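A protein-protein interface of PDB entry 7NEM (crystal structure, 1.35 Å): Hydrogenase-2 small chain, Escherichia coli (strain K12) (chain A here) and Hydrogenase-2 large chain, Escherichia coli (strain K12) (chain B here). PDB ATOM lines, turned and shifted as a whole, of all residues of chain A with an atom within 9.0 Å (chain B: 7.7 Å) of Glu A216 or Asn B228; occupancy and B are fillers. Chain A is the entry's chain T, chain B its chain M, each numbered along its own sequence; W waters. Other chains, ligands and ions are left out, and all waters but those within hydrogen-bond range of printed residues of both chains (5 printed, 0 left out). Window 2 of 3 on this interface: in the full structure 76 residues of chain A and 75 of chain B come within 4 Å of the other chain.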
ATOM      1  N   ARG A 196      11.142  13.390   3.252  1.00  0.00           N
ATOM      2  CA  ARG A 196      10.182  14.477   3.542  1.00  0.00           C
ATOM      3  C   ARG A 196       9.406  14.220   4.835  1.00  0.00           C
ATOM      4  O   ARG A 196       8.556  15.031   5.172  1.00  0.00           O
ATOM      5  CB  ARG A 196       9.231  14.677   2.371  1.00  0.00           C
ATOM      6  CG  ARG A 196      10.004  14.912   1.084  1.00  0.00           C
ATOM      7  CD  ARG A 196       9.170  15.507  -0.034  1.00  0.00           C
ATOM      8  NE  ARG A 196      10.045  15.804  -1.170  1.00  0.00           N
ATOM      9  CZ  ARG A 196       9.721  16.617  -2.171  1.00  0.00           C
ATOM     10  NH1 ARG A 196       8.513  17.153  -2.260  1.00  0.00           N
ATOM     11  NH2 ARG A 196      10.628  16.883  -3.090  1.00  0.00           N
ATOM     12  N   HIS A 199       8.849  17.203   7.143  1.00  0.00           N
ATOM     13  CA  HIS A 199       7.793  18.142   6.702  1.00  0.00           C
ATOM     14  C   HIS A 199       6.436  17.557   7.093  1.00  0.00           C
ATOM     15  O   HIS A 199       5.611  18.318   7.662  1.00  0.00           O
ATOM     16  CB  HIS A 199       7.889  18.329   5.194  1.00  0.00           C
ATOM     17  CG  HIS A 199       9.232  18.843   4.806  1.00  0.00           C
ATOM     18  ND1 HIS A 199       9.746  19.986   5.376  1.00  0.00           N
ATOM     19  CD2 HIS A 199      10.157  18.379   3.910  1.00  0.00           C
ATOM     20  CE1 HIS A 199      10.953  20.203   4.867  1.00  0.00           C
ATOM     21  NE2 HIS A 199      11.234  19.221   3.977  1.00  0.00           N
ATOM     22  N   ARG A 204       4.074  20.619   7.316  1.00  0.00           N
ATOM     23  CA  ARG A 204       4.494  21.351   6.103  1.00  0.00           C
ATOM     24  C   ARG A 204       4.151  20.524   4.870  1.00  0.00           C
ATOM     25  O   ARG A 204       4.825  19.534   4.555  1.00  0.00           O
ATOM     26  CB  ARG A 204       5.972  21.698   6.150  1.00  0.00           C
ATOM     27  CG  ARG A 204       6.366  22.734   7.192  1.00  0.00           C
ATOM     28  CD  ARG A 204       7.820  23.151   7.105  1.00  0.00           C
ATOM     29  NE  ARG A 204       8.736  22.030   7.280  1.00  0.00           N
ATOM     30  CZ  ARG A 204       9.464  21.777   8.364  1.00  0.00           C
ATOM     31  NH1 ARG A 204       9.371  22.550   9.428  1.00  0.00           N
ATOM     32  NH2 ARG A 204      10.308  20.762   8.368  1.00  0.00           N
ATOM     33  N   PHE A 205       3.049  20.877   4.235  1.00  0.00           N
ATOM     34  CA  PHE A 205       2.450  20.079   3.144  1.00  0.00           C
ATOM     35  C   PHE A 205       2.265  20.924   1.886  1.00  0.00           C
ATOM     36  O   PHE A 205       1.764  22.072   1.912  1.00  0.00           O
ATOM     37  CB  PHE A 205       1.058  19.621   3.560  1.00  0.00           C
ATOM     38  CG  PHE A 205       1.048  18.657   4.690  1.00  0.00           C
ATOM     39  CD1 PHE A 205       1.622  17.406   4.573  1.00  0.00           C
ATOM     40  CD2 PHE A 205       0.440  18.984   5.900  1.00  0.00           C
ATOM     41  CE1 PHE A 205       1.641  16.519   5.629  1.00  0.00           C
ATOM     42  CE2 PHE A 205       0.400  18.066   6.932  1.00  0.00           C
ATOM     43  CZ  PHE A 205       1.000  16.843   6.807  1.00  0.00           C
ATOM     44  N   ALA A 206       2.604  20.377   0.718  1.00  0.00           N
ATOM     45  CA  ALA A 206       2.071  20.868  -0.565  1.00  0.00           C
ATOM     46  C   ALA A 206       0.569  20.667  -0.603  1.00  0.00           C
ATOM     47  O   ALA A 206       0.114  19.615  -0.158  1.00  0.00           O
ATOM     48  CB  ALA A 206       2.693  20.099  -1.686  1.00  0.00           C
ATOM     49  N   GLU A 208      -1.258  21.945  -3.619  1.00  0.00           N
ATOM     50  CA  GLU A 208      -1.412  21.827  -5.089  1.00  0.00           C
ATOM     51  C   GLU A 208      -0.008  21.828  -5.695  1.00  0.00           C
ATOM     52  O   GLU A 208       0.875  22.524  -5.162  1.00  0.00           O
ATOM     53  CB  GLU A 208      -2.257  22.994  -5.628  1.00  0.00           C
ATOM     54  CG  GLU A 208      -3.632  23.100  -4.982  1.00  0.00           C
ATOM     55  CD  GLU A 208      -4.602  22.000  -5.342  1.00  0.00           C
ATOM     56  OE1 GLU A 208      -4.326  21.297  -6.335  1.00  0.00           O
ATOM     57  OE2 GLU A 208      -5.580  21.834  -4.621  1.00  0.00           O
ATOM     58  N   GLY A 210       2.891  23.246  -7.735  1.00  0.00           N
ATOM     59  CA  GLY A 210       3.239  24.635  -8.057  1.00  0.00           C
ATOM     60  C   GLY A 210       3.009  25.611  -6.906  1.00  0.00           C
ATOM     61  O   GLY A 210       3.385  26.788  -7.077  1.00  0.00           O
ATOM     62  N   ASP A 211       2.429  25.188  -5.804  1.00  0.00           N
ATOM     63  CA  ASP A 211       2.220  26.117  -4.667  1.00  0.00           C
ATOM     64  C   ASP A 211       3.542  26.308  -3.923  1.00  0.00           C
ATOM     65  O   ASP A 211       4.548  25.726  -4.294  1.00  0.00           O
ATOM     66  CB  ASP A 211       1.050  25.716  -3.780  1.00  0.00           C
ATOM     67  CG  ASP A 211       1.243  24.590  -2.789  1.00  0.00           C
ATOM     68  OD1 ASP A 211       2.411  24.130  -2.623  1.00  0.00           O
ATOM     69  OD2 ASP A 211       0.260  24.229  -2.131  1.00  0.00           O
ATOM     70  N   GLU A 212       3.551  27.191  -2.926  1.00  0.00           N
ATOM     71  CA  GLU A 212       4.836  27.622  -2.329  1.00  0.00           C
ATOM     72  C   GLU A 212       5.432  26.432  -1.599  1.00  0.00           C
ATOM     73  O   GLU A 212       6.631  26.223  -1.769  1.00  0.00           O
ATOM     74  CB  GLU A 212       4.555  28.792  -1.393  1.00  0.00           C
ATOM     75  CG  GLU A 212       5.750  29.507  -0.813  1.00  0.00           C
ATOM     76  CD  GLU A 212       5.172  30.690  -0.035  1.00  0.00           C
ATOM     77  OE1 GLU A 212       4.820  30.498   1.146  1.00  0.00           O
ATOM     78  OE2 GLU A 212       4.902  31.734  -0.681  1.00  0.00           O
ATOM     79  N   GLY A 213       4.647  25.659  -0.880  1.00  0.00           N
ATOM     80  CA  GLY A 213       5.139  24.468  -0.166  1.00  0.00           C
ATOM     81  C   GLY A 213       5.739  23.461  -1.147  1.00  0.00           C
ATOM     82  O   GLY A 213       6.820  22.854  -0.874  1.00  0.00           O
ATOM     83  N   HIS A 214       5.003  23.204  -2.216  1.00  0.00           N
ATOM     84  CA  HIS A 214       5.456  22.266  -3.273  1.00  0.00           C
ATOM     85  C   HIS A 214       6.833  22.713  -3.774  1.00  0.00           C
ATOM     86  O   HIS A 214       7.738  21.884  -3.955  1.00  0.00           O
ATOM     87  CB  HIS A 214       4.409  22.198  -4.345  1.00  0.00           C
ATOM     88  CG  HIS A 214       4.703  21.167  -5.379  1.00  0.00           C
ATOM     89  ND1 HIS A 214       4.849  21.520  -6.682  1.00  0.00           N
ATOM     90  CD2 HIS A 214       4.893  19.827  -5.280  1.00  0.00           C
ATOM     91  CE1 HIS A 214       5.071  20.415  -7.366  1.00  0.00           C
ATOM     92  NE2 HIS A 214       5.111  19.362  -6.543  1.00  0.00           N
ATOM     93  N   ARG A 215       6.980  24.015  -4.000  1.00  0.00           N
ATOM     94  CA  ARG A 215       8.212  24.600  -4.535  1.00  0.00           C
ATOM     95  C   ARG A 215       9.315  24.717  -3.487  1.00  0.00           C
ATOM     96  O   ARG A 215      10.401  25.157  -3.844  1.00  0.00           O
ATOM     97  CB  ARG A 215       7.899  25.910  -5.252  1.00  0.00           C
ATOM     98  CG  ARG A 215       7.110  25.689  -6.533  1.00  0.00           C
ATOM     99  CD  ARG A 215       6.716  27.006  -7.210  1.00  0.00           C
ATOM    100  NE  ARG A 215       7.892  27.732  -7.649  1.00  0.00           N
ATOM    101  CZ  ARG A 215       8.379  28.852  -7.143  1.00  0.00           C
ATOM    102  NH1 ARG A 215       7.656  29.543  -6.258  1.00  0.00           N
ATOM    103  NH2 ARG A 215       9.531  29.328  -7.614  1.00  0.00           N
ATOM    104  N   GLU A 216       9.063  24.287  -2.257  1.00  0.00           N
ATOM    105  CA  GLU A 216      10.095  24.165  -1.203  1.00  0.00           C
ATOM    106  C   GLU A 216      10.361  22.702  -0.885  1.00  0.00           C
ATOM    107  O   GLU A 216      11.108  22.416   0.014  1.00  0.00           O
ATOM    108  CB  GLU A 216       9.702  24.954   0.040  1.00  0.00           C
ATOM    109  CG  GLU A 216       9.667  26.467  -0.177  1.00  0.00           C
ATOM    110  CD  GLU A 216      10.920  27.147  -0.741  1.00  0.00           C
ATOM    111  OE1 GLU A 216      12.091  26.597  -0.629  1.00  0.00           O
ATOM    112  OE2 GLU A 216      10.743  28.242  -1.378  1.00  0.00           O
ATOM    113  N   GLY A 217       9.745  21.764  -1.608  1.00  0.00           N
ATOM    114  CA  GLY A 217      10.043  20.331  -1.372  1.00  0.00           C
ATOM    115  C   GLY A 217       9.362  19.749  -0.152  1.00  0.00           C
ATOM    116  O   GLY A 217       9.846  18.783   0.467  1.00  0.00           O
ATOM    117  N   TRP A 218       8.190  20.274   0.217  1.00  0.00           N
ATOM    118  CA  TRP A 218       7.454  19.779   1.392  1.00  0.00           C
ATOM    119  C   TRP A 218       6.757  18.447   1.098  1.00  0.00           C
ATOM    120  O   TRP A 218       6.794  17.889  -0.005  1.00  0.00           O
ATOM    121  CB  TRP A 218       6.470  20.852   1.834  1.00  0.00           C
ATOM    122  CG  TRP A 218       7.070  22.072   2.428  1.00  0.00           C
ATOM    123  CD1 TRP A 218       8.377  22.354   2.648  1.00  0.00           C
ATOM    124  CD2 TRP A 218       6.321  23.179   2.967  1.00  0.00           C
ATOM    125  NE1 TRP A 218       8.503  23.572   3.283  1.00  0.00           N
ATOM    126  CE2 TRP A 218       7.257  24.102   3.467  1.00  0.00           C
ATOM    127  CE3 TRP A 218       4.952  23.471   3.042  1.00  0.00           C
ATOM    128  CZ2 TRP A 218       6.868  25.297   4.078  1.00  0.00           C
ATOM    129  CZ3 TRP A 218       4.573  24.651   3.649  1.00  0.00           C
ATOM    130  CH2 TRP A 218       5.518  25.543   4.140  1.00  0.00           C
ATOM    131  N   CYS A 219       6.212  17.836   2.135  1.00  0.00           N
ATOM    132  CA  CYS A 219       5.624  16.494   2.079  1.00  0.00           C
ATOM    133  C   CYS A 219       4.397  16.507   1.160  1.00  0.00           C
ATOM    134  O   CYS A 219       3.680  17.548   1.109  1.00  0.00           O
ATOM    135  CB  CYS A 219       5.271  16.030   3.496  1.00  0.00           C
ATOM    136  SG  CYS A 219       4.158  14.604   3.591  1.00  0.00           S
ATOM    137  N   LEU A 220       4.209  15.415   0.422  1.00  0.00           N
ATOM    138  CA  LEU A 220       3.169  15.290  -0.600  1.00  0.00           C
ATOM    139  C   LEU A 220       1.977  14.490  -0.080  1.00  0.00           C
ATOM    140  O   LEU A 220       1.137  14.099  -0.888  1.00  0.00           O
ATOM    141  CB  LEU A 220       3.762  14.696  -1.867  1.00  0.00           C
ATOM    142  CG  LEU A 220       5.021  15.390  -2.361  1.00  0.00           C
ATOM    143  CD1 LEU A 220       5.455  14.729  -3.685  1.00  0.00           C
ATOM    144  CD2 LEU A 220       4.815  16.896  -2.546  1.00  0.00           C
ATOM    145  N   ALA A 249      10.709  12.887  -5.020  1.00  0.00           N
ATOM    146  CA  ALA A 249      11.793  13.890  -5.154  1.00  0.00           C
ATOM    147  C   ALA A 249      11.528  14.780  -6.371  1.00  0.00           C
ATOM    148  O   ALA A 249      11.908  15.967  -6.365  1.00  0.00           O
ATOM    149  CB  ALA A 249      13.136  13.221  -5.268  1.00  0.00           C
ATOM    150  N   ASN B 225       6.597  18.904 -11.571  1.00  0.00           N
ATOM    151  CA  ASN B 225       7.947  19.423 -11.271  1.00  0.00           C
ATOM    152  C   ASN B 225       7.769  20.791 -10.623  1.00  0.00           C
ATOM    153  O   ASN B 225       7.110  21.666 -11.195  1.00  0.00           O
ATOM    154  CB  ASN B 225       8.761  19.575 -12.547  1.00  0.00           C
ATOM    155  CG  ASN B 225       8.799  18.312 -13.364  1.00  0.00           C
ATOM    156  OD1 ASN B 225       7.865  18.059 -14.143  1.00  0.00           O
ATOM    157  ND2 ASN B 225       9.794  17.478 -13.150  1.00  0.00           N
ATOM    158  N   PRO B 226       8.446  21.084  -9.493  1.00  0.00           N
ATOM    159  CA  PRO B 226       8.349  22.398  -8.871  1.00  0.00           C
ATOM    160  C   PRO B 226       9.558  23.223  -9.326  1.00  0.00           C
ATOM    161  O   PRO B 226      10.682  22.920  -8.925  1.00  0.00           O
ATOM    162  CB  PRO B 226       8.339  22.092  -7.373  1.00  0.00           C
ATOM    163  CG  PRO B 226       8.660  20.632  -7.215  1.00  0.00           C
ATOM    164  CD  PRO B 226       9.098  20.132  -8.592  1.00  0.00           C
ATOM    165  N   ILE B 227       9.357  24.240 -10.148  1.00  0.00           N
ATOM    166  CA  ILE B 227      10.473  25.055 -10.674  1.00  0.00           C
ATOM    167  C   ILE B 227      10.824  26.056  -9.601  1.00  0.00           C
ATOM    168  O   ILE B 227       9.966  26.891  -9.237  1.00  0.00           O
ATOM    169  CB  ILE B 227      10.114  25.737 -11.988  1.00  0.00           C
ATOM    170  CG1 ILE B 227       9.951  24.685 -13.087  1.00  0.00           C
ATOM    171  CG2 ILE B 227      11.128  26.810 -12.301  1.00  0.00           C
ATOM    172  CD1 ILE B 227       9.483  25.260 -14.416  1.00  0.00           C
ATOM    173  N   ASN B 228      12.057  26.064  -9.126  1.00  0.00           N
ATOM    174  CA  ASN B 228      12.529  27.070  -8.146  1.00  0.00           C
ATOM    175  C   ASN B 228      14.049  27.048  -8.203  1.00  0.00           C
ATOM    176  O   ASN B 228      14.649  26.173  -7.579  1.00  0.00           O
ATOM    177  CB  ASN B 228      11.979  26.834  -6.754  1.00  0.00           C
ATOM    178  CG  ASN B 228      12.405  27.883  -5.758  1.00  0.00           C
ATOM    179  OD1 ASN B 228      13.170  28.789  -6.098  1.00  0.00           O
ATOM    180  ND2 ASN B 228      11.941  27.701  -4.544  1.00  0.00           N
ATOM    181  N   LEU B 229      14.646  27.987  -8.904  1.00  0.00           N
ATOM    182  CA  LEU B 229      16.120  27.998  -9.091  1.00  0.00           C
ATOM    183  C   LEU B 229      16.827  27.995  -7.757  1.00  0.00           C
ATOM    184  O   LEU B 229      17.981  27.494  -7.723  1.00  0.00           O
ATOM    185  CB  LEU B 229      16.533  29.226  -9.898  1.00  0.00           C
ATOM    186  CG  LEU B 229      16.094  29.242 -11.364  1.00  0.00           C
ATOM    187  CD1 LEU B 229      16.595  30.520 -12.031  1.00  0.00           C
ATOM    188  CD2 LEU B 229      16.557  28.035 -12.159  1.00  0.00           C
ATOM    189  N   ASP B 230      16.194  28.534  -6.717  1.00  0.00           N
ATOM    190  CA  ASP B 230      16.798  28.771  -5.384  1.00  0.00           C
ATOM    191  C   ASP B 230      16.301  27.774  -4.350  1.00  0.00           C
ATOM    192  O   ASP B 230      16.615  27.941  -3.186  1.00  0.00           O
ATOM    193  CB  ASP B 230      16.542  30.220  -5.021  1.00  0.00           C
ATOM    194  CG  ASP B 230      17.271  31.138  -5.972  1.00  0.00           C
ATOM    195  OD1 ASP B 230      18.525  31.109  -6.049  1.00  0.00           O
ATOM    196  OD2 ASP B 230      16.543  31.909  -6.633  1.00  0.00           O
ATOM    197  N   GLY B 231      15.548  26.743  -4.778  1.00  0.00           N
ATOM    198  CA  GLY B 231      14.954  25.773  -3.875  1.00  0.00           C
ATOM    199  C   GLY B 231      15.800  24.538  -3.673  1.00  0.00           C
ATOM    200  O   GLY B 231      16.309  23.978  -4.617  1.00  0.00           O
ATOM    201  N   LEU B 232      15.850  24.078  -2.451  1.00  0.00           N
ATOM    202  CA  LEU B 232      16.452  22.783  -2.075  1.00  0.00           C
ATOM    203  C   LEU B 232      15.415  21.709  -2.341  1.00  0.00           C
ATOM    204  O   LEU B 232      14.261  21.872  -1.952  1.00  0.00           O
ATOM    205  CB  LEU B 232      16.905  22.894  -0.610  1.00  0.00           C
ATOM    206  CG  LEU B 232      17.681  21.700  -0.083  1.00  0.00           C
ATOM    207  CD1 LEU B 232      18.679  22.189   0.973  1.00  0.00           C
ATOM    208  CD2 LEU B 232      16.793  20.621   0.460  1.00  0.00           C
ATOM    209  N   GLY B 233      15.817  20.628  -3.005  1.00  0.00           N
ATOM    210  CA  GLY B 233      14.927  19.471  -3.183  1.00  0.00           C
ATOM    211  C   GLY B 233      13.941  19.583  -4.300  1.00  0.00           C
ATOM    212  O   GLY B 233      13.104  18.685  -4.399  1.00  0.00           O
ATOM    213  N   VAL B 234      14.034  20.619  -5.124  1.00  0.00           N
ATOM    214  CA  VAL B 234      13.107  20.859  -6.254  1.00  0.00           C
ATOM    215  C   VAL B 234      13.898  21.082  -7.539  1.00  0.00           C
ATOM    216  O   VAL B 234      15.137  20.841  -7.562  1.00  0.00           O
ATOM    217  CB  VAL B 234      12.166  22.021  -5.902  1.00  0.00           C
ATOM    218  CG1 VAL B 234      11.346  21.713  -4.639  1.00  0.00           C
ATOM    219  CG2 VAL B 234      12.856  23.369  -5.777  1.00  0.00           C
ATOM    220  N   LEU B 235      13.220  21.473  -8.606  1.00  0.00           N
ATOM    221  CA  LEU B 235      13.841  21.606  -9.929  1.00  0.00           C
ATOM    222  C   LEU B 235      14.547  22.965  -9.937  1.00  0.00           C
ATOM    223  O   LEU B 235      13.944  24.020 -10.238  1.00  0.00           O
ATOM    224  CB  LEU B 235      12.809  21.446 -11.049  1.00  0.00           C
ATOM    225  CG  LEU B 235      13.381  21.509 -12.461  1.00  0.00           C
ATOM    226  CD1 LEU B 235      14.430  20.445 -12.678  1.00  0.00           C
ATOM    227  CD2 LEU B 235      12.236  21.326 -13.435  1.00  0.00           C
ATOM    228  N   ASN B 236      15.824  22.934  -9.579  1.00  0.00           N
ATOM    229  CA  ASN B 236      16.636  24.151  -9.449  1.00  0.00           C
ATOM    230  C   ASN B 236      17.684  24.197 -10.557  1.00  0.00           C
ATOM    231  O   ASN B 236      17.669  23.391 -11.482  1.00  0.00           O
ATOM    232  CB  ASN B 236      17.205  24.230  -8.045  1.00  0.00           C
ATOM    233  CG  ASN B 236      18.065  23.037  -7.704  1.00  0.00           C
ATOM    234  OD1 ASN B 236      18.674  22.457  -8.597  1.00  0.00           O
ATOM    235  ND2 ASN B 236      18.195  22.707  -6.440  1.00  0.00           N
ATOM    236  N   LEU B 237      18.610  25.149 -10.501  1.00  0.00           N
ATOM    237  CA  LEU B 237      19.526  25.303 -11.642  1.00  0.00           C
ATOM    238  C   LEU B 237      20.490  24.105 -11.681  1.00  0.00           C
ATOM    239  O   LEU B 237      20.877  23.640 -12.757  1.00  0.00           O
ATOM    240  CB  LEU B 237      20.291  26.617 -11.544  1.00  0.00           C
ATOM    241  CG  LEU B 237      21.163  26.932 -12.758  1.00  0.00           C
ATOM    242  CD1 LEU B 237      20.355  26.932 -14.055  1.00  0.00           C
ATOM    243  CD2 LEU B 237      21.846  28.276 -12.565  1.00  0.00           C
ATOM    244  N   GLU B 238      20.901  23.603 -10.541  1.00  0.00           N
ATOM    245  CA  GLU B 238      21.811  22.424 -10.487  1.00  0.00           C
ATOM    246  C   GLU B 238      21.142  21.219 -11.181  1.00  0.00           C
ATOM    247  O   GLU B 238      21.792  20.525 -11.994  1.00  0.00           O
ATOM    248  CB  GLU B 238      22.176  22.108  -9.040  1.00  0.00           C
ATOM    249  CG  GLU B 238      23.033  20.859  -8.878  1.00  0.00           C
ATOM    250  CD  GLU B 238      22.235  19.565  -8.860  1.00  0.00           C
ATOM    251  OE1 GLU B 238      21.098  19.550  -8.345  1.00  0.00           O
ATOM    252  OE2 GLU B 238      22.756  18.544  -9.328  1.00  0.00           O
ATOM    253  N   LEU B 240      18.761  21.329 -13.467  1.00  0.00           N
ATOM    254  CA  LEU B 240      18.636  21.651 -14.900  1.00  0.00           C
ATOM    255  C   LEU B 240      19.989  21.447 -15.584  1.00  0.00           C
ATOM    256  O   LEU B 240      20.048  20.845 -16.660  1.00  0.00           O
ATOM    257  CB  LEU B 240      18.119  23.090 -15.055  1.00  0.00           C
ATOM    258  CG  LEU B 240      16.635  23.259 -14.689  1.00  0.00           C
ATOM    259  CD1 LEU B 240      16.263  24.716 -14.465  1.00  0.00           C
ATOM    260  CD2 LEU B 240      15.741  22.661 -15.780  1.00  0.00           C
ATOM    261  N   ILE B 450      12.288  30.630 -17.372  1.00  0.00           N
ATOM    262  CA  ILE B 450      12.454  30.719 -15.901  1.00  0.00           C
ATOM    263  C   ILE B 450      13.194  32.041 -15.593  1.00  0.00           C
ATOM    264  O   ILE B 450      12.829  32.677 -14.628  1.00  0.00           O
ATOM    265  CB  ILE B 450      13.197  29.475 -15.366  1.00  0.00           C
ATOM    266  CG1 ILE B 450      12.386  28.209 -15.616  1.00  0.00           C
ATOM    267  CG2 ILE B 450      13.542  29.659 -13.893  1.00  0.00           C
ATOM    268  CD1 ILE B 450      13.184  26.933 -15.398  1.00  0.00           C
ATOM    269  N   HIS B 455       7.744  30.765 -13.147  1.00  0.00           N
ATOM    270  CA  HIS B 455       7.984  29.435 -12.538  1.00  0.00           C
ATOM    271  C   HIS B 455       6.688  28.604 -12.558  1.00  0.00           C
ATOM    272  O   HIS B 455       6.638  27.603 -11.863  1.00  0.00           O
ATOM    273  CB  HIS B 455       8.520  29.606 -11.119  1.00  0.00           C
ATOM    274  CG  HIS B 455       7.591  30.338 -10.216  1.00  0.00           C
ATOM    275  ND1 HIS B 455       7.878  31.587  -9.725  1.00  0.00           N
ATOM    276  CD2 HIS B 455       6.389  30.007  -9.710  1.00  0.00           C
ATOM    277  CE1 HIS B 455       6.893  31.997  -8.964  1.00  0.00           C
ATOM    278  NE2 HIS B 455       5.974  31.053  -8.944  1.00  0.00           N
ATOM    279  N   THR B 457       3.824  26.018 -13.489  1.00  0.00           N
ATOM    280  CA  THR B 457       3.870  24.632 -14.040  1.00  0.00           C
ATOM    281  C   THR B 457       2.518  23.924 -14.047  1.00  0.00           C
ATOM    282  O   THR B 457       2.415  22.882 -14.696  1.00  0.00           O
ATOM    283  CB  THR B 457       4.816  23.814 -13.153  1.00  0.00           C
ATOM    284  OG1 THR B 457       4.506  24.091 -11.786  1.00  0.00           O
ATOM    285  CG2 THR B 457       6.263  24.143 -13.401  1.00  0.00           C
HETATM  286  O   HOH W   1      12.678  29.694  -2.320  1.00  0.00           O
HETATM  287  O   HOH W   2      10.620  18.307  -5.692  1.00  0.00           O
HETATM  288  O   HOH W   3      13.621  24.403  -0.404  1.00  0.00           O
HETATM  289  O   HOH W   4      14.306  28.221  -0.722  1.00  0.00           O
HETATM  290  O   HOH W   5      14.015  16.221  -3.525  1.00  0.00           O
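O of Gly B233 sits at hydrogen-bond distance from NH2 of Arg A196 (3.3 Å).
The guanidinium group of Arg A215 is in hydrogen-bond range of the backbone carbonyl oxygen of Ile B227.
O of Arg A215 lies within hydrogen-bond range of ND2 of Asn B228 (3.1 Å).
The side-chain carboxylate of Glu A216 is in hydrogen-bond range of the side-chain amide nitrogen of Asn B228.
The guanidinium group (NE) of Arg A196 sits close to the backbone carbonyl oxygen (O) of Gly A217, 3.4 Å away.
O of Trp A218 is in hydrogen-bond range of NH1 of Arg A196 (2.9 Å).
The backbone NH of Gly A210 sits at hydrogen-bond distance from a ring nitrogen (ND1) of His A214.
The side-chain carboxylate (OD1) of Asp A211 lies within hydrogen-bond range of the backbone NH (N) of His A214 (2.8 Å).
The backbone NH (N) of Leu B235 sits at hydrogen-bond distance from the backbone carbonyl oxygen (O) of Pro B226 (2.9 Å).
The backbone NH (N) of Asn B228 is in hydrogen-bond range of the backbone carbonyl oxygen (O) of Leu B235 (3.0 Å).
Among the printed residues, pairs that only touch across the chains: Gly A210 with Thr B457, His A214 with Pro B226, His A214 with Val B234, Arg A215 with Pro B226, Arg A215 with Val B234, Arg A215 with His B455, Glu A216 with Leu B232, Gly A217 with Val B234 and Ala A249 with Gly B233.
Printed residues of chain B within 4 Å of Glu A216: Asn B228 (3.4 Å) and Leu B232 (3.8 Å).
Asn B228 touches just these residues of chain A: Arg A215 and Glu A216.
Of the printed residues of chain A, Thr B457 touches Gly A210 (3.98 Å).
Of the printed residues of chain A, Ile B227 touches Arg A215 (2.7 Å).
Printed residues of chain A within 4 Å of Val B234: His A214 (3.7 Å), Arg A215 (3.6 Å) and Gly A217 (3.4 Å).
Of the printed residues of chain B, His A214 touches Pro B226 (3.5 Å) and Val B234 (3.7 Å).
The nearest residue of chain A that does not touch Asn B228 is Glu A212 (6.2 Å).
The nearest printed residue of chain B that does not touch Arg A215 is Gly B231 (4.6 Å).
Hydrophobic or aromatic side chains of chain A that line the printed part of chain B: His A214.
Of the 18 printed residues of chain B, 8 touch a printed residue of chain A.
Hydrophobic or aromatic side chains of chain B that line the printed part of chain A: Pro B226, Val B234 and His B455.
Among the printed residues, 13 pairs touch across the chains.
Among the printed residues, no Asp or Glu carboxylate lies within 4 Å of a Lys or Arg side-chain nitrogen of the other chain.
Water W1 bridges the side-chain carboxylate of Glu A216 and the side-chain amide nitrogen of Asn B228.
Water W3 bridges OE1 of Glu A216 and O of Leu B232.
Water W4 bridges the side-chain carboxylate (OE1) of Glu A216 (2.7 Å) and the backbone carbonyl oxygen (O) of Asp B230 (3.4 Å).
Water W2 lies within hydrogen-bond range of O of Ala A249, O of Gly B233 and NH2 of Arg A196.
Water W5 lies within hydrogen-bond range of the backbone carbonyl oxygen of Gly B233 (2.8 Å) and the guanidinium group of Arg A196 (3.5 Å).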
